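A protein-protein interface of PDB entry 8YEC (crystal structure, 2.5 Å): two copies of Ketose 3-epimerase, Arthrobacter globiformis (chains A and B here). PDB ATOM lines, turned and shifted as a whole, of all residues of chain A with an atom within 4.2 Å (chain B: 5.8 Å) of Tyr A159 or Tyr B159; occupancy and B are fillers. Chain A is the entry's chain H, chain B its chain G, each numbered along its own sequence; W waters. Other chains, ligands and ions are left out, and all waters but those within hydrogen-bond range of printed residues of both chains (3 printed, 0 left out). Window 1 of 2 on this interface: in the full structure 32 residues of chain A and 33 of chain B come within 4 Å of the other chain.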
ATOM      1  N   LYS A 119     -28.759   4.889  34.202  1.00  0.00           N
ATOM      2  CA  LYS A 119     -28.700   5.246  32.803  1.00  0.00           C
ATOM      3  C   LYS A 119     -27.299   4.978  32.276  1.00  0.00           C
ATOM      4  O   LYS A 119     -26.405   4.582  33.036  1.00  0.00           O
ATOM      5  CB  LYS A 119     -29.032   6.725  32.613  1.00  0.00           C
ATOM      6  CG  LYS A 119     -28.062   7.684  33.278  1.00  0.00           C
ATOM      7  CD  LYS A 119     -28.069   9.026  32.599  1.00  0.00           C
ATOM      8  CE  LYS A 119     -27.030   9.957  33.178  1.00  0.00           C
ATOM      9  NZ  LYS A 119     -26.889  11.183  32.357  1.00  0.00           N
ATOM     10  N   LYS A 120     -27.130   5.219  30.964  1.00  0.00           N
ATOM     11  CA  LYS A 120     -25.842   5.120  30.299  1.00  0.00           C
ATOM     12  C   LYS A 120     -25.177   6.505  30.292  1.00  0.00           C
ATOM     13  O   LYS A 120     -25.423   7.335  29.421  1.00  0.00           O
ATOM     14  CB  LYS A 120     -26.023   4.498  28.909  1.00  0.00           C
ATOM     15  CG  LYS A 120     -24.762   4.362  28.062  1.00  0.00           C
ATOM     16  CD  LYS A 120     -23.576   3.785  28.803  1.00  0.00           C
ATOM     17  CE  LYS A 120     -22.351   3.660  27.931  1.00  0.00           C
ATOM     18  NZ  LYS A 120     -22.064   4.902  27.173  1.00  0.00           N
ATOM     19  N   ASN A 157     -24.106  -2.657  36.436  1.00  0.00           N
ATOM     20  CA  ASN A 157     -23.064  -2.717  35.425  1.00  0.00           C
ATOM     21  C   ASN A 157     -22.801  -1.345  34.797  1.00  0.00           C
ATOM     22  O   ASN A 157     -23.538  -0.383  34.978  1.00  0.00           O
ATOM     23  CB  ASN A 157     -23.426  -3.726  34.324  1.00  0.00           C
ATOM     24  CG  ASN A 157     -24.648  -3.320  33.514  1.00  0.00           C
ATOM     25  OD1 ASN A 157     -24.648  -2.301  32.825  1.00  0.00           O
ATOM     26  ND2 ASN A 157     -25.716  -4.091  33.612  1.00  0.00           N
ATOM     27  N   ARG A 158     -21.750  -1.313  33.972  1.00  0.00           N
ATOM     28  CA  ARG A 158     -21.181  -0.090  33.434  1.00  0.00           C
ATOM     29  C   ARG A 158     -22.202   0.722  32.647  1.00  0.00           C
ATOM     30  O   ARG A 158     -22.017   1.921  32.505  1.00  0.00           O
ATOM     31  CB  ARG A 158     -19.991  -0.419  32.531  1.00  0.00           C
ATOM     32  CG  ARG A 158     -20.404  -1.132  31.261  1.00  0.00           C
ATOM     33  CD  ARG A 158     -19.225  -1.753  30.560  1.00  0.00           C
ATOM     34  NE  ARG A 158     -18.457  -2.597  31.453  1.00  0.00           N
ATOM     35  CZ  ARG A 158     -17.165  -2.867  31.304  1.00  0.00           C
ATOM     36  NH1 ARG A 158     -16.537  -2.536  30.191  1.00  0.00           N
ATOM     37  NH2 ARG A 158     -16.502  -3.479  32.271  1.00  0.00           N
ATOM     38  N   TYR A 159     -23.253   0.080  32.130  1.00  0.00           N
ATOM     39  CA  TYR A 159     -24.231   0.746  31.280  1.00  0.00           C
ATOM     40  C   TYR A 159     -25.397   1.353  32.062  1.00  0.00           C
ATOM     41  O   TYR A 159     -26.232   2.027  31.457  1.00  0.00           O
ATOM     42  CB  TYR A 159     -24.836  -0.240  30.277  1.00  0.00           C
ATOM     43  CG  TYR A 159     -23.842  -0.876  29.348  1.00  0.00           C
ATOM     44  CD1 TYR A 159     -23.482  -2.203  29.491  1.00  0.00           C
ATOM     45  CD2 TYR A 159     -23.273  -0.158  28.318  1.00  0.00           C
ATOM     46  CE1 TYR A 159     -22.571  -2.802  28.642  1.00  0.00           C
ATOM     47  CE2 TYR A 159     -22.375  -0.751  27.444  1.00  0.00           C
ATOM     48  CZ  TYR A 159     -22.024  -2.079  27.603  1.00  0.00           C
ATOM     49  OH  TYR A 159     -21.114  -2.689  26.770  1.00  0.00           O
ATOM     50  N   GLU A 160     -25.492   1.056  33.365  1.00  0.00           N
ATOM     51  CA  GLU A 160     -26.587   1.532  34.197  1.00  0.00           C
ATOM     52  C   GLU A 160     -26.104   2.429  35.347  1.00  0.00           C
ATOM     53  O   GLU A 160     -26.939   2.966  36.071  1.00  0.00           O
ATOM     54  CB  GLU A 160     -27.370   0.343  34.753  1.00  0.00           C
ATOM     55  CG  GLU A 160     -28.153  -0.455  33.709  1.00  0.00           C
ATOM     56  CD  GLU A 160     -29.153  -1.438  34.322  1.00  0.00           C
ATOM     57  OE1 GLU A 160     -29.721  -1.104  35.380  1.00  0.00           O
ATOM     58  OE2 GLU A 160     -29.375  -2.537  33.765  1.00  0.00           O
ATOM     59  N   THR A 161     -24.777   2.561  35.531  1.00  0.00           N
ATOM     60  CA  THR A 161     -24.172   3.587  36.374  1.00  0.00           C
ATOM     61  C   THR A 161     -22.680   3.670  36.060  1.00  0.00           C
ATOM     62  O   THR A 161     -22.084   2.706  35.573  1.00  0.00           O
ATOM     63  CB  THR A 161     -24.327   3.287  37.869  1.00  0.00           C
ATOM     64  OG1 THR A 161     -23.931   4.427  38.633  1.00  0.00           O
ATOM     65  CG2 THR A 161     -23.485   2.107  38.294  1.00  0.00           C
ATOM     66  N   TYR A 189     -27.207 -10.941  37.584  1.00  0.00           N
ATOM     67  CA  TYR A 189     -27.188 -10.418  36.223  1.00  0.00           C
ATOM     68  C   TYR A 189     -26.051  -9.416  36.045  1.00  0.00           C
ATOM     69  O   TYR A 189     -25.404  -9.395  35.008  1.00  0.00           O
ATOM     70  CB  TYR A 189     -28.522  -9.757  35.885  1.00  0.00           C
ATOM     71  CG  TYR A 189     -28.497  -8.871  34.667  1.00  0.00           C
ATOM     72  CD1 TYR A 189     -28.479  -9.414  33.397  1.00  0.00           C
ATOM     73  CD2 TYR A 189     -28.502  -7.490  34.782  1.00  0.00           C
ATOM     74  CE1 TYR A 189     -28.455  -8.611  32.269  1.00  0.00           C
ATOM     75  CE2 TYR A 189     -28.483  -6.673  33.663  1.00  0.00           C
ATOM     76  CZ  TYR A 189     -28.455  -7.234  32.397  1.00  0.00           C
ATOM     77  OH  TYR A 189     -28.446  -6.442  31.264  1.00  0.00           O
ATOM     78  N   LEU A 263     -33.990  -0.017  31.049  1.00  0.00           N
ATOM     79  CA  LEU A 263     -33.256  -1.259  31.171  1.00  0.00           C
ATOM     80  C   LEU A 263     -32.955  -1.905  29.820  1.00  0.00           C
ATOM     81  O   LEU A 263     -32.204  -2.877  29.786  1.00  0.00           O
ATOM     82  CB  LEU A 263     -34.062  -2.199  32.065  1.00  0.00           C
ATOM     83  CG  LEU A 263     -34.156  -1.759  33.519  1.00  0.00           C
ATOM     84  CD1 LEU A 263     -34.805  -2.851  34.337  1.00  0.00           C
ATOM     85  CD2 LEU A 263     -32.780  -1.389  34.080  1.00  0.00           C
ATOM     86  N   LYS B 119     -25.273   2.761  20.625  1.00  0.00           N
ATOM     87  CA  LYS B 119     -25.540   3.453  21.878  1.00  0.00           C
ATOM     88  C   LYS B 119     -26.618   2.723  22.686  1.00  0.00           C
ATOM     89  O   LYS B 119     -27.128   1.679  22.284  1.00  0.00           O
ATOM     90  CB  LYS B 119     -25.953   4.891  21.566  1.00  0.00           C
ATOM     91  CG  LYS B 119     -27.203   5.007  20.697  1.00  0.00           C
ATOM     92  CD  LYS B 119     -27.889   6.348  20.834  1.00  0.00           C
ATOM     93  CE  LYS B 119     -29.270   6.326  20.222  1.00  0.00           C
ATOM     94  NZ  LYS B 119     -29.908   7.658  20.268  1.00  0.00           N
ATOM     95  N   LYS B 120     -26.950   3.286  23.849  1.00  0.00           N
ATOM     96  CA  LYS B 120     -28.082   2.832  24.636  1.00  0.00           C
ATOM     97  C   LYS B 120     -29.318   3.558  24.112  1.00  0.00           C
ATOM     98  O   LYS B 120     -29.573   4.709  24.442  1.00  0.00           O
ATOM     99  CB  LYS B 120     -27.830   3.082  26.132  1.00  0.00           C
ATOM    100  CG  LYS B 120     -29.045   2.895  27.031  1.00  0.00           C
ATOM    101  CD  LYS B 120     -29.781   1.573  26.783  1.00  0.00           C
ATOM    102  CE  LYS B 120     -30.741   1.206  27.893  1.00  0.00           C
ATOM    103  NZ  LYS B 120     -31.540   2.375  28.328  1.00  0.00           N
ATOM    104  N   TYR B 121     -30.080   2.880  23.263  1.00  0.00           N
ATOM    105  CA  TYR B 121     -31.356   3.415  22.819  1.00  0.00           C
ATOM    106  C   TYR B 121     -32.383   3.405  23.948  1.00  0.00           C
ATOM    107  O   TYR B 121     -32.344   2.570  24.849  1.00  0.00           O
ATOM    108  CB  TYR B 121     -31.897   2.591  21.653  1.00  0.00           C
ATOM    109  CG  TYR B 121     -31.204   2.801  20.329  1.00  0.00           C
ATOM    110  CD1 TYR B 121     -30.008   2.177  20.032  1.00  0.00           C
ATOM    111  CD2 TYR B 121     -31.772   3.609  19.362  1.00  0.00           C
ATOM    112  CE1 TYR B 121     -29.408   2.333  18.797  1.00  0.00           C
ATOM    113  CE2 TYR B 121     -31.182   3.780  18.126  1.00  0.00           C
ATOM    114  CZ  TYR B 121     -29.999   3.140  17.840  1.00  0.00           C
ATOM    115  OH  TYR B 121     -29.443   3.351  16.613  1.00  0.00           O
ATOM    116  N   ASN B 157     -24.932  -6.249  22.785  1.00  0.00           N
ATOM    117  CA  ASN B 157     -25.950  -6.384  23.814  1.00  0.00           C
ATOM    118  C   ASN B 157     -26.976  -5.254  23.736  1.00  0.00           C
ATOM    119  O   ASN B 157     -26.848  -4.315  22.959  1.00  0.00           O
ATOM    120  CB  ASN B 157     -25.296  -6.450  25.194  1.00  0.00           C
ATOM    121  CG  ASN B 157     -24.615  -5.162  25.598  1.00  0.00           C
ATOM    122  OD1 ASN B 157     -25.268  -4.201  25.968  1.00  0.00           O
ATOM    123  ND2 ASN B 157     -23.300  -5.135  25.546  1.00  0.00           N
ATOM    124  N   ARG B 158     -27.999  -5.345  24.585  1.00  0.00           N
ATOM    125  CA  ARG B 158     -29.122  -4.421  24.600  1.00  0.00           C
ATOM    126  C   ARG B 158     -28.699  -2.967  24.828  1.00  0.00           C
ATOM    127  O   ARG B 158     -29.391  -2.062  24.367  1.00  0.00           O
ATOM    128  CB  ARG B 158     -30.079  -4.840  25.718  1.00  0.00           C
ATOM    129  CG  ARG B 158     -29.425  -4.882  27.094  1.00  0.00           C
ATOM    130  CD  ARG B 158     -30.260  -5.632  28.111  1.00  0.00           C
ATOM    131  NE  ARG B 158     -30.438  -7.021  27.720  1.00  0.00           N
ATOM    132  CZ  ARG B 158     -31.340  -7.840  28.241  1.00  0.00           C
ATOM    133  NH1 ARG B 158     -32.110  -7.439  29.236  1.00  0.00           N
ATOM    134  NH2 ARG B 158     -31.479  -9.064  27.760  1.00  0.00           N
ATOM    135  N   TYR B 159     -27.595  -2.730  25.560  1.00  0.00           N
ATOM    136  CA  TYR B 159     -27.193  -1.372  25.923  1.00  0.00           C
ATOM    137  C   TYR B 159     -26.414  -0.671  24.811  1.00  0.00           C
ATOM    138  O   TYR B 159     -26.079   0.490  24.989  1.00  0.00           O
ATOM    139  CB  TYR B 159     -26.318  -1.357  27.179  1.00  0.00           C
ATOM    140  CG  TYR B 159     -26.929  -1.993  28.403  1.00  0.00           C
ATOM    141  CD1 TYR B 159     -27.963  -1.388  29.093  1.00  0.00           C
ATOM    142  CD2 TYR B 159     -26.464  -3.201  28.870  1.00  0.00           C
ATOM    143  CE1 TYR B 159     -28.526  -1.978  30.208  1.00  0.00           C
ATOM    144  CE2 TYR B 159     -27.020  -3.807  29.975  1.00  0.00           C
ATOM    145  CZ  TYR B 159     -28.062  -3.204  30.642  1.00  0.00           C
ATOM    146  OH  TYR B 159     -28.590  -3.839  31.735  1.00  0.00           O
ATOM    147  N   GLU B 160     -26.112  -1.366  23.699  1.00  0.00           N
ATOM    148  CA  GLU B 160     -25.324  -0.814  22.592  1.00  0.00           C
ATOM    149  C   GLU B 160     -26.055  -0.825  21.236  1.00  0.00           C
ATOM    150  O   GLU B 160     -25.575  -0.218  20.285  1.00  0.00           O
ATOM    151  CB  GLU B 160     -23.992  -1.570  22.474  1.00  0.00           C
ATOM    152  CG  GLU B 160     -22.908  -1.010  23.372  1.00  0.00           C
ATOM    153  CD  GLU B 160     -21.584  -1.752  23.313  1.00  0.00           C
ATOM    154  OE1 GLU B 160     -21.108  -2.049  22.198  1.00  0.00           O
ATOM    155  OE2 GLU B 160     -21.030  -2.044  24.392  1.00  0.00           O
ATOM    156  N   THR B 161     -27.170  -1.558  21.127  1.00  0.00           N
ATOM    157  CA  THR B 161     -28.089  -1.480  20.003  1.00  0.00           C
ATOM    158  C   THR B 161     -29.422  -2.081  20.428  1.00  0.00           C
ATOM    159  O   THR B 161     -29.471  -2.847  21.389  1.00  0.00           O
ATOM    160  CB  THR B 161     -27.617  -2.275  18.777  1.00  0.00           C
ATOM    161  OG1 THR B 161     -28.535  -2.057  17.703  1.00  0.00           O
ATOM    162  CG2 THR B 161     -27.563  -3.764  19.044  1.00  0.00           C
ATOM    163  N   ASN B 165     -29.363  -8.158  18.833  1.00  0.00           N
ATOM    164  CA  ASN B 165     -28.845  -8.545  20.135  1.00  0.00           C
ATOM    165  C   ASN B 165     -28.502 -10.041  20.235  1.00  0.00           C
ATOM    166  O   ASN B 165     -27.956 -10.481  21.246  1.00  0.00           O
ATOM    167  CB  ASN B 165     -29.854  -8.182  21.232  1.00  0.00           C
ATOM    168  CG  ASN B 165     -30.037  -6.692  21.449  1.00  0.00           C
ATOM    169  OD1 ASN B 165     -31.137  -6.245  21.761  1.00  0.00           O
ATOM    170  ND2 ASN B 165     -28.972  -5.921  21.321  1.00  0.00           N
ATOM    171  N   TYR B 189     -18.003 -11.362  24.805  1.00  0.00           N
ATOM    172  CA  TYR B 189     -18.428 -10.396  25.805  1.00  0.00           C
ATOM    173  C   TYR B 189     -19.922 -10.143  25.720  1.00  0.00           C
ATOM    174  O   TYR B 189     -20.620 -10.219  26.721  1.00  0.00           O
ATOM    175  CB  TYR B 189     -17.727  -9.055  25.599  1.00  0.00           C
ATOM    176  CG  TYR B 189     -18.352  -7.885  26.319  1.00  0.00           C
ATOM    177  CD1 TYR B 189     -18.392  -7.826  27.703  1.00  0.00           C
ATOM    178  CD2 TYR B 189     -18.873  -6.812  25.619  1.00  0.00           C
ATOM    179  CE1 TYR B 189     -18.927  -6.732  28.368  1.00  0.00           C
ATOM    180  CE2 TYR B 189     -19.417  -5.717  26.270  1.00  0.00           C
ATOM    181  CZ  TYR B 189     -19.441  -5.673  27.650  1.00  0.00           C
ATOM    182  OH  TYR B 189     -19.970  -4.595  28.315  1.00  0.00           O
ATOM    183  N   HIS B 190     -20.392  -9.827  24.517  1.00  0.00           N
ATOM    184  CA  HIS B 190     -21.811  -9.607  24.289  1.00  0.00           C
ATOM    185  C   HIS B 190     -22.595 -10.914  24.344  1.00  0.00           C
ATOM    186  O   HIS B 190     -23.735 -10.929  24.781  1.00  0.00           O
ATOM    187  CB  HIS B 190     -22.009  -8.929  22.937  1.00  0.00           C
ATOM    188  CG  HIS B 190     -21.398  -7.567  22.859  1.00  0.00           C
ATOM    189  ND1 HIS B 190     -21.938  -6.473  23.502  1.00  0.00           N
ATOM    190  CD2 HIS B 190     -20.319  -7.129  22.214  1.00  0.00           C
ATOM    191  CE1 HIS B 190     -21.211  -5.408  23.234  1.00  0.00           C
ATOM    192  NE2 HIS B 190     -20.204  -5.787  22.480  1.00  0.00           N
ATOM    193  N   ILE B 193     -24.003 -11.982  27.637  1.00  0.00           N
ATOM    194  CA  ILE B 193     -25.208 -11.358  28.142  1.00  0.00           C
ATOM    195  C   ILE B 193     -26.425 -11.977  27.463  1.00  0.00           C
ATOM    196  O   ILE B 193     -27.264 -12.578  28.128  1.00  0.00           O
ATOM    197  CB  ILE B 193     -25.128  -9.827  27.984  1.00  0.00           C
ATOM    198  CG1 ILE B 193     -23.890  -9.282  28.699  1.00  0.00           C
ATOM    199  CG2 ILE B 193     -26.393  -9.201  28.511  1.00  0.00           C
ATOM    200  CD1 ILE B 193     -23.570  -7.836  28.452  1.00  0.00           C
ATOM    201  N   GLU B 194     -26.506 -11.886  26.135  1.00  0.00           N
ATOM    202  CA  GLU B 194     -27.780 -12.057  25.444  1.00  0.00           C
ATOM    203  C   GLU B 194     -28.121 -13.520  25.108  1.00  0.00           C
ATOM    204  O   GLU B 194     -29.300 -13.879  25.075  1.00  0.00           O
ATOM    205  CB  GLU B 194     -27.785 -11.210  24.169  1.00  0.00           C
ATOM    206  CG  GLU B 194     -27.627  -9.708  24.424  1.00  0.00           C
ATOM    207  CD  GLU B 194     -28.757  -9.085  25.227  1.00  0.00           C
ATOM    208  OE1 GLU B 194     -29.835  -9.686  25.266  1.00  0.00           O
ATOM    209  OE2 GLU B 194     -28.559  -8.014  25.826  1.00  0.00           O
ATOM    210  N   ARG B 219     -14.126  -7.129  30.257  1.00  0.00           N
ATOM    211  CA  ARG B 219     -13.333  -6.553  29.173  1.00  0.00           C
ATOM    212  C   ARG B 219     -11.883  -6.284  29.590  1.00  0.00           C
ATOM    213  O   ARG B 219     -11.207  -5.482  28.948  1.00  0.00           O
ATOM    214  CB  ARG B 219     -14.005  -5.284  28.642  1.00  0.00           C
ATOM    215  CG  ARG B 219     -15.420  -5.500  28.121  1.00  0.00           C
ATOM    216  CD  ARG B 219     -15.493  -5.655  26.614  1.00  0.00           C
ATOM    217  NE  ARG B 219     -16.091  -4.477  26.012  1.00  0.00           N
ATOM    218  CZ  ARG B 219     -16.646  -4.451  24.806  1.00  0.00           C
ATOM    219  NH1 ARG B 219     -16.531  -5.487  23.989  1.00  0.00           N
ATOM    220  NH2 ARG B 219     -17.321  -3.377  24.422  1.00  0.00           N
ATOM    221  N   MET B 262     -18.302   5.962  24.942  1.00  0.00           N
ATOM    222  CA  MET B 262     -19.398   5.237  24.312  1.00  0.00           C
ATOM    223  C   MET B 262     -19.576   3.833  24.915  1.00  0.00           C
ATOM    224  O   MET B 262     -20.703   3.337  25.045  1.00  0.00           O
ATOM    225  CB  MET B 262     -19.144   5.114  22.805  1.00  0.00           C
ATOM    226  CG  MET B 262     -19.302   6.410  22.048  1.00  0.00           C
ATOM    227  SD  MET B 262     -19.196   6.157  20.255  1.00  0.00           S
ATOM    228  CE  MET B 262     -20.880   6.551  19.778  1.00  0.00           C
ATOM    229  N   LEU B 263     -18.458   3.195  25.290  1.00  0.00           N
ATOM    230  CA  LEU B 263     -18.453   1.817  25.754  1.00  0.00           C
ATOM    231  C   LEU B 263     -18.531   1.708  27.276  1.00  0.00           C
ATOM    232  O   LEU B 263     -18.532   0.590  27.797  1.00  0.00           O
ATOM    233  CB  LEU B 263     -17.170   1.148  25.255  1.00  0.00           C
ATOM    234  CG  LEU B 263     -17.136   0.834  23.764  1.00  0.00           C
ATOM    235  CD1 LEU B 263     -16.064  -0.196  23.469  1.00  0.00           C
ATOM    236  CD2 LEU B 263     -18.502   0.364  23.279  1.00  0.00           C
ATOM    237  N   GLY B 264     -18.593   2.846  27.981  1.00  0.00           N
ATOM    238  CA  GLY B 264     -18.601   2.872  29.439  1.00  0.00           C
ATOM    239  C   GLY B 264     -17.351   2.236  30.054  1.00  0.00           C
ATOM    240  O   GLY B 264     -17.437   1.352  30.905  1.00  0.00           O
ATOM    241  N   TRP B 266     -15.191   2.859  32.496  1.00  0.00           N
ATOM    242  CA  TRP B 266     -15.030   3.674  33.690  1.00  0.00           C
ATOM    243  C   TRP B 266     -13.922   3.155  34.614  1.00  0.00           C
ATOM    244  O   TRP B 266     -13.452   3.905  35.470  1.00  0.00           O
ATOM    245  CB  TRP B 266     -16.334   3.732  34.484  1.00  0.00           C
ATOM    246  CG  TRP B 266     -17.605   3.901  33.711  1.00  0.00           C
ATOM    247  CD1 TRP B 266     -18.749   3.171  33.875  1.00  0.00           C
ATOM    248  CD2 TRP B 266     -17.899   4.877  32.702  1.00  0.00           C
ATOM    249  NE1 TRP B 266     -19.732   3.622  33.041  1.00  0.00           N
ATOM    250  CE2 TRP B 266     -19.243   4.670  32.306  1.00  0.00           C
ATOM    251  CE3 TRP B 266     -17.174   5.912  32.105  1.00  0.00           C
ATOM    252  CZ2 TRP B 266     -19.870   5.458  31.336  1.00  0.00           C
ATOM    253  CZ3 TRP B 266     -17.792   6.683  31.140  1.00  0.00           C
ATOM    254  CH2 TRP B 266     -19.119   6.452  30.754  1.00  0.00           C
HETATM  255  O   HOH W   1     -18.246  -2.237  27.292  1.00  0.00           O
HETATM  256  O   HOH W   2     -31.282  -4.822  31.375  1.00  0.00           O
HETATM  257  O   HOH W   3     -29.911   4.866  29.608  1.00  0.00           O
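The side-chain hydroxyl of Tyr B189 is in hydrogen-bond range of the side-chain hydroxyl of Tyr A159, at 2.7 Å. OH of Tyr B159 is in hydrogen-bond range of OH of Tyr A189 (2.6 Å). OE2 of Glu A160 sits at hydrogen-bond distance from OH of Tyr B159 (2.5 Å). The side-chain hydroxyl of Tyr B159 sits at hydrogen-bond distance from the side-chain amide nitrogen of Asn A157, at 3.4 Å. O of Arg A158 is in hydrogen-bond range of NE1 of Trp B266 (2.9 Å). O of Met B262 sits at hydrogen-bond distance from NZ of Lys A120. The side-chain hydroxyl (OH) of Tyr A159 sits at hydrogen-bond distance from the side-chain carboxylate (OE2) of Glu B160, 2.5 Å away.
The side-chain amide nitrogen of Asn B157 is in hydrogen-bond range of a ring nitrogen (ND1) of His B190 (2.8 Å). N of Arg B158 sits close to ND2 of Asn B165, 3.5 Å away. The backbone NH (N) of Lys B119 is in hydrogen-bond range of the backbone carbonyl oxygen (O) of Glu B160, at 3.0 Å. O of Tyr B159 sits close to N of Lys B120. The backbone NH (N) of Lys A119 lies within hydrogen-bond range of the backbone carbonyl oxygen (O) of Glu A160, 3.2 Å away. The side-chain amide oxygen (OD1) of Asn A157 sits at hydrogen-bond distance from the backbone NH (N) of Tyr A159 (2.8 Å).
Lys B120 touches Lys A120 (CB to CB, 3.6 Å). Tyr B189 touches Arg A158. NH1 of Arg A158 touches CG of Arg B219, at 3.8 Å. Gly B264 touches Arg A158. Tyr A159 touches Asn B157. CD1 of Tyr A159 touches CD2 of Tyr B159 (3.2 Å). Trp B266 touches Thr A161 (NE1 to O, 3.6 Å). Tyr A189 touches Arg B158 (OH to CD, 3.7 Å). O of Leu A263 touches CD of Arg B158, at 3.8 Å. Leu A263 touches Tyr B159.
Tyr A159 touches just these residues of chain B: Asn B157 (3.5 Å), Tyr B159 (3.2 Å), Glu B160 (2.5 Å) and Tyr B189 (2.7 Å). Tyr B159 touches five residues of chain A. Of the printed residues of chain A, Asn B157 touches Tyr A159. Of the printed residues of chain A, Leu B263 touches Arg A158 (3.7 Å). The nearest residue of chain B that does not touch Tyr A159 is Leu B263 (4.1 Å). The nearest printed residue of chain B that does not touch Lys A120 is Leu B263 (4.3 Å).
Of the 9 printed residues of chain A, 8 touch a printed residue of chain B. Hydrophobic or aromatic side chains of chain A that line the printed part of chain B: Tyr A159 and Tyr A189. Along chain A the printed residues that touch a printed residue of chain B span positions 120 to 263. Printed residues of chain B that touch a printed residue of chain A: Lys B120, Asn B157, Arg B158, Tyr B159, Glu B160, Tyr B189, Arg B219, Met B262, Leu B263, Gly B264 and Trp B266. Among the printed residues, 19 pairs touch across the chains. Among the printed residues, no Asp or Glu carboxylate lies within 4 Å of a Lys or Arg side-chain nitrogen of the other chain.
Tyr A159 touches its own counterpart, Tyr B159. Tyr A159 touches Glu B160, and with the chains exchanged Glu A160 touches Tyr B159. Tyr A159 touches Tyr B189, and with the chains exchanged Tyr A189 touches Tyr B159. Leu A263 touches Tyr B159, but with the chains exchanged Tyr A159 does not touch Leu B263 (4.1 Å).
Water W2 lies within hydrogen-bond range of O of Leu A263, OH of Tyr B159, OH of Tyr A189 and NH1 of Arg B158. Water W1 lies within hydrogen-bond range of the backbone carbonyl oxygen (O) of Leu B263 (2.9 Å), the side-chain hydroxyl (OH) of Tyr A159 (2.9 Å), the side-chain hydroxyl (OH) of Tyr B189 (3.1 Å), the guanidinium group (NH2) of Arg B219 (3.2 Å) and the guanidinium group (NH1) of Arg A158 (3.4 Å). Water W3 lies within hydrogen-bond range of the backbone NH (N) of Lys A120 and the side-chain amino group (NZ) of Lys B120.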
